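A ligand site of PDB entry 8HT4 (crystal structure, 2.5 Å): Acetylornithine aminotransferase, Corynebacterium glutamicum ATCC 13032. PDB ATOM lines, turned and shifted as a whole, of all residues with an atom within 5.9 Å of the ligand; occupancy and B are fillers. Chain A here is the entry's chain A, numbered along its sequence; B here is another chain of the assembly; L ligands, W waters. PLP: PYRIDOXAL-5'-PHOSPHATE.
An oxygen (O3) of the ligand is in hydrogen-bond range of the side-chain amide nitrogen (NE2) of Gln 227 (3.1 Å).
N1 of the ligand is in hydrogen-bond range of OD2 of Asp 224 (2.8 Å).
The side-chain hydroxyl (OG1) of Thr 282 of chain B is in hydrogen-bond range of an oxygen (O3P) of the ligand, at 3.0 Å.
The side-chain amino group (NZ) of Lys 253 sits at hydrogen-bond distance from an oxygen (O3) of the ligand (2.9 Å).
The backbone NH (N) of Gly 110 sits at hydrogen-bond distance from an oxygen (O3P) of the ligand (3.3 Å).
The backbone NH of Thr 282 of chain B lies close to an oxygen (O1P) of the ligand (3.1 Å).
The backbone NH of Ala 111 lies within hydrogen-bond range of an oxygen (O2P) of the ligand (2.9 Å).
Water W2 lies within hydrogen-bond range of O3P of the ligand (2.7 Å), N of Lys 253 (2.9 Å) and OG1 of Thr 282 of chain B (3.0 Å).
O of Phe 136 sits close to N1 of the ligand (3.3 Å).
CB of Ser 109 touches O2P of the ligand, at 3.6 Å.
ND2 of Asn 114 touches C6 of the ligand, 3.9 Å away.
His 137 touches the ligand (O to C6, 3.6 Å).
CA of Gly 138 touches C5A of the ligand (3.996 Å).
OE1 of Glu 191 touches C2A of the ligand, at 3.4 Å.
CG1 of Val 226 touches C4 of the ligand, 3.6 Å away.
Thr 281 of chain B touches the ligand.
Hydrophobic or aromatic side chains that line the ligand: Ala 111, Phe 136 and Val 226.
Of the 26 residues printed, 14 come within 4 Å of the ligand.
The side-chain hydroxyl (OG1) of Thr 281 of chain B lies within hydrogen-bond range of the side-chain amide nitrogen (ND2) of Asn 108 of chain B, 3.5 Å away.
ND2 of Asn 114 is in hydrogen-bond range of O of His 137 (2.9 Å).
ND1 of His 137 sits at hydrogen-bond distance from OD2 of Asp 224, 2.8 Å away.
The side-chain carboxylate of Glu 191 is in hydrogen-bond range of the backbone NH of Phe 136 (3.0 Å).
The side-chain hydroxyl of Ser 109 is in hydrogen-bond range of the side-chain carboxylate of Glu 112 of chain B (2.5 Å).
The side-chain carboxylate (OE1) of Glu 191 lies within hydrogen-bond range of the backbone NH (N) of Gly 195 (2.9 Å).
ND2 of Asn 114 sits at hydrogen-bond distance from OD2 of Asp 224 (2.8 Å).
The backbone NH of Glu 112 of chain A is in hydrogen-bond range of the side-chain hydroxyl of Ser 109, 3.1 Å away.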
ATOM      1  N   ILE A  45     -11.416 -13.907  16.282  1.00  0.00           N
ATOM      2  CA  ILE A  45     -12.471 -14.864  16.725  1.00  0.00           C
ATOM      3  C   ILE A  45     -13.756 -14.093  17.014  1.00  0.00           C
ATOM      4  O   ILE A  45     -14.158 -14.081  18.142  1.00  0.00           O
ATOM      5  CB  ILE A  45     -12.039 -15.894  17.799  1.00  0.00           C
ATOM      6  CG1 ILE A  45     -10.608 -16.390  17.597  1.00  0.00           C
ATOM      7  CG2 ILE A  45     -13.006 -17.053  17.879  1.00  0.00           C
ATOM      8  CD1 ILE A  45      -9.899 -16.718  18.876  1.00  0.00           C
ATOM      9  N   ASN A 108     -15.883  -8.569  32.278  1.00  0.00           N
ATOM     10  CA  ASN A 108     -14.712  -8.268  31.402  1.00  0.00           C
ATOM     11  C   ASN A 108     -14.457  -9.346  30.336  1.00  0.00           C
ATOM     12  O   ASN A 108     -13.543  -9.134  29.517  1.00  0.00           O
ATOM     13  CB  ASN A 108     -13.439  -8.049  32.233  1.00  0.00           C
ATOM     14  CG  ASN A 108     -13.679  -7.026  33.314  1.00  0.00           C
ATOM     15  OD1 ASN A 108     -13.880  -5.853  33.005  1.00  0.00           O
ATOM     16  ND2 ASN A 108     -13.790  -7.480  34.549  1.00  0.00           N
ATOM     17  N   SER A 109     -15.186 -10.444  30.327  1.00  0.00           N
ATOM     18  CA  SER A 109     -14.995 -11.504  29.310  1.00  0.00           C
ATOM     19  C   SER A 109     -16.268 -12.342  29.215  1.00  0.00           C
ATOM     20  O   SER A 109     -17.118 -12.231  30.108  1.00  0.00           O
ATOM     21  CB  SER A 109     -13.831 -12.349  29.702  1.00  0.00           C
ATOM     22  OG  SER A 109     -14.016 -12.883  30.997  1.00  0.00           O
ATOM     23  N   GLY A 110     -16.365 -13.181  28.186  1.00  0.00           N
ATOM     24  CA  GLY A 110     -17.376 -14.268  28.130  1.00  0.00           C
ATOM     25  C   GLY A 110     -17.259 -15.181  29.344  1.00  0.00           C
ATOM     26  O   GLY A 110     -18.291 -15.471  29.949  1.00  0.00           O
ATOM     27  N   ALA A 111     -16.047 -15.599  29.717  1.00  0.00           N
ATOM     28  CA  ALA A 111     -15.847 -16.497  30.859  1.00  0.00           C
ATOM     29  C   ALA A 111     -16.528 -15.887  32.080  1.00  0.00           C
ATOM     30  O   ALA A 111     -17.444 -16.517  32.659  1.00  0.00           O
ATOM     31  CB  ALA A 111     -14.380 -16.723  31.089  1.00  0.00           C
ATOM     32  N   GLU A 112     -16.158 -14.661  32.416  1.00  0.00           N
ATOM     33  CA  GLU A 112     -16.726 -13.956  33.608  1.00  0.00           C
ATOM     34  C   GLU A 112     -18.261 -13.876  33.473  1.00  0.00           C
ATOM     35  O   GLU A 112     -18.969 -14.002  34.521  1.00  0.00           O
ATOM     36  CB  GLU A 112     -16.086 -12.587  33.762  1.00  0.00           C
ATOM     37  CG  GLU A 112     -14.760 -12.650  34.486  1.00  0.00           C
ATOM     38  CD  GLU A 112     -14.154 -11.307  34.842  1.00  0.00           C
ATOM     39  OE1 GLU A 112     -14.586 -10.280  34.269  1.00  0.00           O
ATOM     40  OE2 GLU A 112     -13.235 -11.291  35.710  1.00  0.00           O
ATOM     41  N   ASN A 114     -20.310 -15.943  31.773  1.00  0.00           N
ATOM     42  CA  ASN A 114     -20.881 -17.281  32.051  1.00  0.00           C
ATOM     43  C   ASN A 114     -20.671 -17.658  33.528  1.00  0.00           C
ATOM     44  O   ASN A 114     -21.436 -18.517  34.012  1.00  0.00           O
ATOM     45  CB  ASN A 114     -20.374 -18.366  31.088  1.00  0.00           C
ATOM     46  CG  ASN A 114     -21.067 -18.270  29.747  1.00  0.00           C
ATOM     47  OD1 ASN A 114     -22.274 -18.000  29.678  1.00  0.00           O
ATOM     48  ND2 ASN A 114     -20.309 -18.453  28.683  1.00  0.00           N
ATOM     49  N   PHE A 136     -18.940 -24.513  24.337  1.00  0.00           N
ATOM     50  CA  PHE A 136     -17.795 -23.787  24.924  1.00  0.00           C
ATOM     51  C   PHE A 136     -18.356 -22.553  25.654  1.00  0.00           C
ATOM     52  O   PHE A 136     -19.095 -21.787  25.033  1.00  0.00           O
ATOM     53  CB  PHE A 136     -16.745 -23.499  23.833  1.00  0.00           C
ATOM     54  CG  PHE A 136     -15.604 -22.681  24.341  1.00  0.00           C
ATOM     55  CD1 PHE A 136     -14.619 -23.267  25.124  1.00  0.00           C
ATOM     56  CD2 PHE A 136     -15.567 -21.303  24.129  1.00  0.00           C
ATOM     57  CE1 PHE A 136     -13.586 -22.508  25.654  1.00  0.00           C
ATOM     58  CE2 PHE A 136     -14.531 -20.547  24.667  1.00  0.00           C
ATOM     59  CZ  PHE A 136     -13.560 -21.145  25.438  1.00  0.00           C
ATOM     60  N   HIS A 137     -18.134 -22.446  26.965  1.00  0.00           N
ATOM     61  CA  HIS A 137     -18.603 -21.312  27.806  1.00  0.00           C
ATOM     62  C   HIS A 137     -17.408 -20.576  28.454  1.00  0.00           C
ATOM     63  O   HIS A 137     -17.608 -19.486  29.065  1.00  0.00           O
ATOM     64  CB  HIS A 137     -19.669 -21.826  28.767  1.00  0.00           C
ATOM     65  CG  HIS A 137     -20.884 -22.343  28.071  1.00  0.00           C
ATOM     66  ND1 HIS A 137     -21.642 -21.565  27.209  1.00  0.00           N
ATOM     67  CD2 HIS A 137     -21.480 -23.562  28.106  1.00  0.00           C
ATOM     68  CE1 HIS A 137     -22.635 -22.290  26.720  1.00  0.00           C
ATOM     69  NE2 HIS A 137     -22.560 -23.519  27.251  1.00  0.00           N
ATOM     70  N   GLY A 138     -16.175 -21.085  28.295  1.00  0.00           N
ATOM     71  CA  GLY A 138     -14.964 -20.372  28.734  1.00  0.00           C
ATOM     72  C   GLY A 138     -14.057 -21.250  29.577  1.00  0.00           C
ATOM     73  O   GLY A 138     -14.354 -22.433  29.667  1.00  0.00           O
ATOM     74  N   ARG A 139     -13.022 -20.655  30.186  1.00  0.00           N
ATOM     75  CA  ARG A 139     -11.824 -21.364  30.716  1.00  0.00           C
ATOM     76  C   ARG A 139     -11.595 -21.105  32.215  1.00  0.00           C
ATOM     77  O   ARG A 139     -10.684 -21.763  32.788  1.00  0.00           O
ATOM     78  CB  ARG A 139     -10.568 -20.934  29.962  1.00  0.00           C
ATOM     79  CG  ARG A 139     -10.652 -21.052  28.450  1.00  0.00           C
ATOM     80  CD  ARG A 139     -10.183 -22.400  27.973  1.00  0.00           C
ATOM     81  NE  ARG A 139      -9.403 -22.356  26.740  1.00  0.00           N
ATOM     82  CZ  ARG A 139      -8.528 -23.302  26.402  1.00  0.00           C
ATOM     83  NH1 ARG A 139      -8.292 -24.328  27.221  1.00  0.00           N
ATOM     84  NH2 ARG A 139      -7.870 -23.226  25.263  1.00  0.00           N
ATOM     85  N   GLU A 191     -25.355 -22.719  23.219  1.00  0.00           N
ATOM     86  CA  GLU A 191     -24.940 -21.692  22.256  1.00  0.00           C
ATOM     87  C   GLU A 191     -26.074 -21.676  21.207  1.00  0.00           C
ATOM     88  O   GLU A 191     -26.409 -22.772  20.777  1.00  0.00           O
ATOM     89  CB  GLU A 191     -23.603 -22.022  21.610  1.00  0.00           C
ATOM     90  CG  GLU A 191     -22.391 -21.728  22.459  1.00  0.00           C
ATOM     91  CD  GLU A 191     -21.163 -22.431  21.921  1.00  0.00           C
ATOM     92  OE1 GLU A 191     -20.451 -21.839  21.112  1.00  0.00           O
ATOM     93  OE2 GLU A 191     -20.945 -23.578  22.307  1.00  0.00           O
ATOM     94  N   GLY A 195     -19.960 -22.464  18.286  1.00  0.00           N
ATOM     95  CA  GLY A 195     -18.852 -21.791  17.575  1.00  0.00           C
ATOM     96  C   GLY A 195     -17.614 -22.637  17.559  1.00  0.00           C
ATOM     97  O   GLY A 195     -17.133 -22.939  16.450  1.00  0.00           O
ATOM     98  N   GLU A 196     -17.124 -23.022  18.742  1.00  0.00           N
ATOM     99  CA  GLU A 196     -15.858 -23.774  18.970  1.00  0.00           C
ATOM    100  C   GLU A 196     -15.859 -25.045  18.093  1.00  0.00           C
ATOM    101  O   GLU A 196     -14.902 -25.203  17.310  1.00  0.00           O
ATOM    102  CB  GLU A 196     -15.700 -24.084  20.470  1.00  0.00           C
ATOM    103  CG  GLU A 196     -14.518 -24.991  20.816  1.00  0.00           C
ATOM    104  CD  GLU A 196     -13.183 -24.274  20.915  1.00  0.00           C
ATOM    105  OE1 GLU A 196     -13.199 -23.045  21.067  1.00  0.00           O
ATOM    106  OE2 GLU A 196     -12.130 -24.956  20.833  1.00  0.00           O
ATOM    107  N   ASP A 224     -25.816 -18.445  25.661  1.00  0.00           N
ATOM    108  CA  ASP A 224     -24.453 -17.912  25.433  1.00  0.00           C
ATOM    109  C   ASP A 224     -24.449 -17.219  24.080  1.00  0.00           C
ATOM    110  O   ASP A 224     -24.364 -17.918  23.038  1.00  0.00           O
ATOM    111  CB  ASP A 224     -23.395 -19.006  25.524  1.00  0.00           C
ATOM    112  CG  ASP A 224     -21.986 -18.458  25.510  1.00  0.00           C
ATOM    113  OD1 ASP A 224     -21.776 -17.411  24.872  1.00  0.00           O
ATOM    114  OD2 ASP A 224     -21.092 -19.099  26.107  1.00  0.00           O
ATOM    115  N   GLU A 225     -24.468 -15.882  24.091  1.00  0.00           N
ATOM    116  CA  GLU A 225     -24.419 -15.053  22.850  1.00  0.00           C
ATOM    117  C   GLU A 225     -23.055 -14.362  22.722  1.00  0.00           C
ATOM    118  O   GLU A 225     -22.924 -13.501  21.842  1.00  0.00           O
ATOM    119  CB  GLU A 225     -25.582 -14.058  22.829  1.00  0.00           C
ATOM    120  CG  GLU A 225     -26.924 -14.741  22.634  1.00  0.00           C
ATOM    121  CD  GLU A 225     -27.456 -14.768  21.202  1.00  0.00           C
ATOM    122  OE1 GLU A 225     -26.725 -14.331  20.278  1.00  0.00           O
ATOM    123  OE2 GLU A 225     -28.598 -15.218  21.024  1.00  0.00           O
ATOM    124  N   VAL A 226     -22.045 -14.798  23.494  1.00  0.00           N
ATOM    125  CA  VAL A 226     -20.648 -14.268  23.404  1.00  0.00           C
ATOM    126  C   VAL A 226     -20.230 -14.182  21.919  1.00  0.00           C
ATOM    127  O   VAL A 226     -19.624 -13.167  21.541  1.00  0.00           O
ATOM    128  CB  VAL A 226     -19.637 -15.109  24.216  1.00  0.00           C
ATOM    129  CG1 VAL A 226     -18.217 -14.628  23.982  1.00  0.00           C
ATOM    130  CG2 VAL A 226     -19.919 -15.120  25.714  1.00  0.00           C
ATOM    131  N   GLN A 227     -20.430 -15.200  21.092  1.00  0.00           N
ATOM    132  CA  GLN A 227     -19.952 -15.166  19.680  1.00  0.00           C
ATOM    133  C   GLN A 227     -21.082 -14.788  18.717  1.00  0.00           C
ATOM    134  O   GLN A 227     -20.814 -14.021  17.790  1.00  0.00           O
ATOM    135  CB  GLN A 227     -19.297 -16.499  19.301  1.00  0.00           C
ATOM    136  CG  GLN A 227     -18.836 -16.606  17.858  1.00  0.00           C
ATOM    137  CD  GLN A 227     -17.891 -17.774  17.668  1.00  0.00           C
ATOM    138  OE1 GLN A 227     -17.491 -18.080  16.555  1.00  0.00           O
ATOM    139  NE2 GLN A 227     -17.543 -18.420  18.759  1.00  0.00           N
ATOM    140  N   ALA A 252     -20.007 -11.044  25.284  1.00  0.00           N
ATOM    141  CA  ALA A 252     -18.630 -10.516  25.325  1.00  0.00           C
ATOM    142  C   ALA A 252     -18.156 -10.281  23.887  1.00  0.00           C
ATOM    143  O   ALA A 252     -18.872  -9.609  23.190  1.00  0.00           O
ATOM    144  CB  ALA A 252     -17.731 -11.446  26.110  1.00  0.00           C
ATOM    145  N   LYS A 253     -16.963 -10.699  23.487  1.00  0.00           N
ATOM    146  CA  LYS A 253     -16.394 -10.514  22.114  1.00  0.00           C
ATOM    147  C   LYS A 253     -16.827  -9.224  21.386  1.00  0.00           C
ATOM    148  O   LYS A 253     -16.231  -8.189  21.661  1.00  0.00           O
ATOM    149  CB  LYS A 253     -16.545 -11.779  21.279  1.00  0.00           C
ATOM    150  CG  LYS A 253     -16.045 -13.039  21.959  1.00  0.00           C
ATOM    151  CD  LYS A 253     -15.232 -13.946  21.107  1.00  0.00           C
ATOM    152  CE  LYS A 253     -16.031 -15.124  20.620  1.00  0.00           C
ATOM    153  NZ  LYS A 253     -15.154 -16.288  20.369  1.00  0.00           N
ATOM    154  N   ASN B 108      -8.074 -10.413  32.163  1.00  0.00           N
ATOM    155  CA  ASN B 108      -8.831  -9.132  32.165  1.00  0.00           C
ATOM    156  C   ASN B 108      -9.234  -8.691  33.586  1.00  0.00           C
ATOM    157  O   ASN B 108      -9.998  -7.689  33.648  1.00  0.00           O
ATOM    158  CB  ASN B 108     -10.053  -9.266  31.272  1.00  0.00           C
ATOM    159  CG  ASN B 108      -9.694  -9.936  29.956  1.00  0.00           C
ATOM    160  OD1 ASN B 108      -8.918  -9.400  29.184  1.00  0.00           O
ATOM    161  ND2 ASN B 108     -10.223 -11.121  29.727  1.00  0.00           N
ATOM    162  N   GLU B 112      -9.821 -13.532  37.098  1.00  0.00           N
ATOM    163  CA  GLU B 112      -9.282 -14.346  35.963  1.00  0.00           C
ATOM    164  C   GLU B 112      -7.835 -14.752  36.247  1.00  0.00           C
ATOM    165  O   GLU B 112      -7.451 -15.894  35.871  1.00  0.00           O
ATOM    166  CB  GLU B 112      -9.379 -13.600  34.628  1.00  0.00           C
ATOM    167  CG  GLU B 112     -10.766 -13.657  33.986  1.00  0.00           C
ATOM    168  CD  GLU B 112     -10.881 -13.264  32.527  1.00  0.00           C
ATOM    169  OE1 GLU B 112     -10.032 -12.495  32.057  1.00  0.00           O
ATOM    170  OE2 GLU B 112     -11.803 -13.765  31.844  1.00  0.00           O
ATOM    171  N   GLY B 280      -6.568 -20.275  28.392  1.00  0.00           N
ATOM    172  CA  GLY B 280      -6.763 -19.259  27.353  1.00  0.00           C
ATOM    173  C   GLY B 280      -7.841 -18.249  27.740  1.00  0.00           C
ATOM    174  O   GLY B 280      -8.485 -18.439  28.809  1.00  0.00           O
ATOM    175  N   THR B 281      -8.004 -17.229  26.900  1.00  0.00           N
ATOM    176  CA  THR B 281      -8.986 -16.108  26.997  1.00  0.00           C
ATOM    177  C   THR B 281      -8.837 -15.295  25.699  1.00  0.00           C
ATOM    178  O   THR B 281      -7.676 -15.151  25.229  1.00  0.00           O
ATOM    179  CB  THR B 281      -8.806 -15.330  28.317  1.00  0.00           C
ATOM    180  OG1 THR B 281      -9.852 -14.358  28.472  1.00  0.00           O
ATOM    181  CG2 THR B 281      -7.457 -14.654  28.438  1.00  0.00           C
ATOM    182  N   THR B 282      -9.923 -14.822  25.103  1.00  0.00           N
ATOM    183  CA  THR B 282      -9.870 -14.049  23.834  1.00  0.00           C
ATOM    184  C   THR B 282      -9.142 -12.730  24.112  1.00  0.00           C
ATOM    185  O   THR B 282      -8.131 -12.495  23.405  1.00  0.00           O
ATOM    186  CB  THR B 282     -11.259 -13.801  23.229  1.00  0.00           C
ATOM    187  OG1 THR B 282     -11.914 -12.872  24.096  1.00  0.00           O
ATOM    188  CG2 THR B 282     -12.096 -15.061  23.088  1.00  0.00           C
ATOM    189  N   PHE B 283      -9.586 -11.971  25.127  1.00  0.00           N
ATOM    190  CA  PHE B 283      -9.179 -10.548  25.356  1.00  0.00           C
ATOM    191  C   PHE B 283      -7.767 -10.442  25.947  1.00  0.00           C
ATOM    192  O   PHE B 283      -7.191  -9.331  25.818  1.00  0.00           O
ATOM    193  CB  PHE B 283     -10.118  -9.793  26.292  1.00  0.00           C
ATOM    194  CG  PHE B 283     -11.496  -9.566  25.730  1.00  0.00           C
ATOM    195  CD1 PHE B 283     -11.669  -9.204  24.385  1.00  0.00           C
ATOM    196  CD2 PHE B 283     -12.616  -9.729  26.535  1.00  0.00           C
ATOM    197  CE1 PHE B 283     -12.943  -9.007  23.885  1.00  0.00           C
ATOM    198  CE2 PHE B 283     -13.881  -9.544  26.016  1.00  0.00           C
ATOM    199  CZ  PHE B 283     -14.045  -9.183  24.691  1.00  0.00           C
HETATM  200  N1  PLP L   1     -18.602 -18.520  24.946  1.00  0.00           N
HETATM  201  C2  PLP L   1     -18.407 -18.505  23.633  1.00  0.00           C
HETATM  202  C2A PLP L   1     -19.493 -18.971  22.723  1.00  0.00           C
HETATM  203  C3  PLP L   1     -17.203 -18.047  23.111  1.00  0.00           C
HETATM  204  O3  PLP L   1     -17.059 -18.050  21.768  1.00  0.00           O
HETATM  205  C4  PLP L   1     -16.199 -17.598  23.977  1.00  0.00           C
HETATM  206  C4A PLP L   1     -14.934 -17.134  23.420  1.00  0.00           C
HETATM  207  C5  PLP L   1     -16.447 -17.624  25.367  1.00  0.00           C
HETATM  208  C6  PLP L   1     -17.647 -18.093  25.790  1.00  0.00           C
HETATM  209  C5A PLP L   1     -15.424 -17.181  26.373  1.00  0.00           C
HETATM  210  O4P PLP L   1     -15.106 -15.762  26.246  1.00  0.00           O
HETATM  211  P   PLP L   1     -13.674 -15.254  26.720  1.00  0.00           P
HETATM  212  O1P PLP L   1     -12.688 -16.055  25.945  1.00  0.00           O
HETATM  213  O2P PLP L   1     -13.598 -15.556  28.177  1.00  0.00           O
HETATM  214  O3P PLP L   1     -13.624 -13.797  26.429  1.00  0.00           O
HETATM  215  O   HOH W   1     -11.930 -17.917  22.382  1.00  0.00           O
HETATM  216  O   HOH W   2     -14.776 -12.156  24.618  1.00  0.00           O
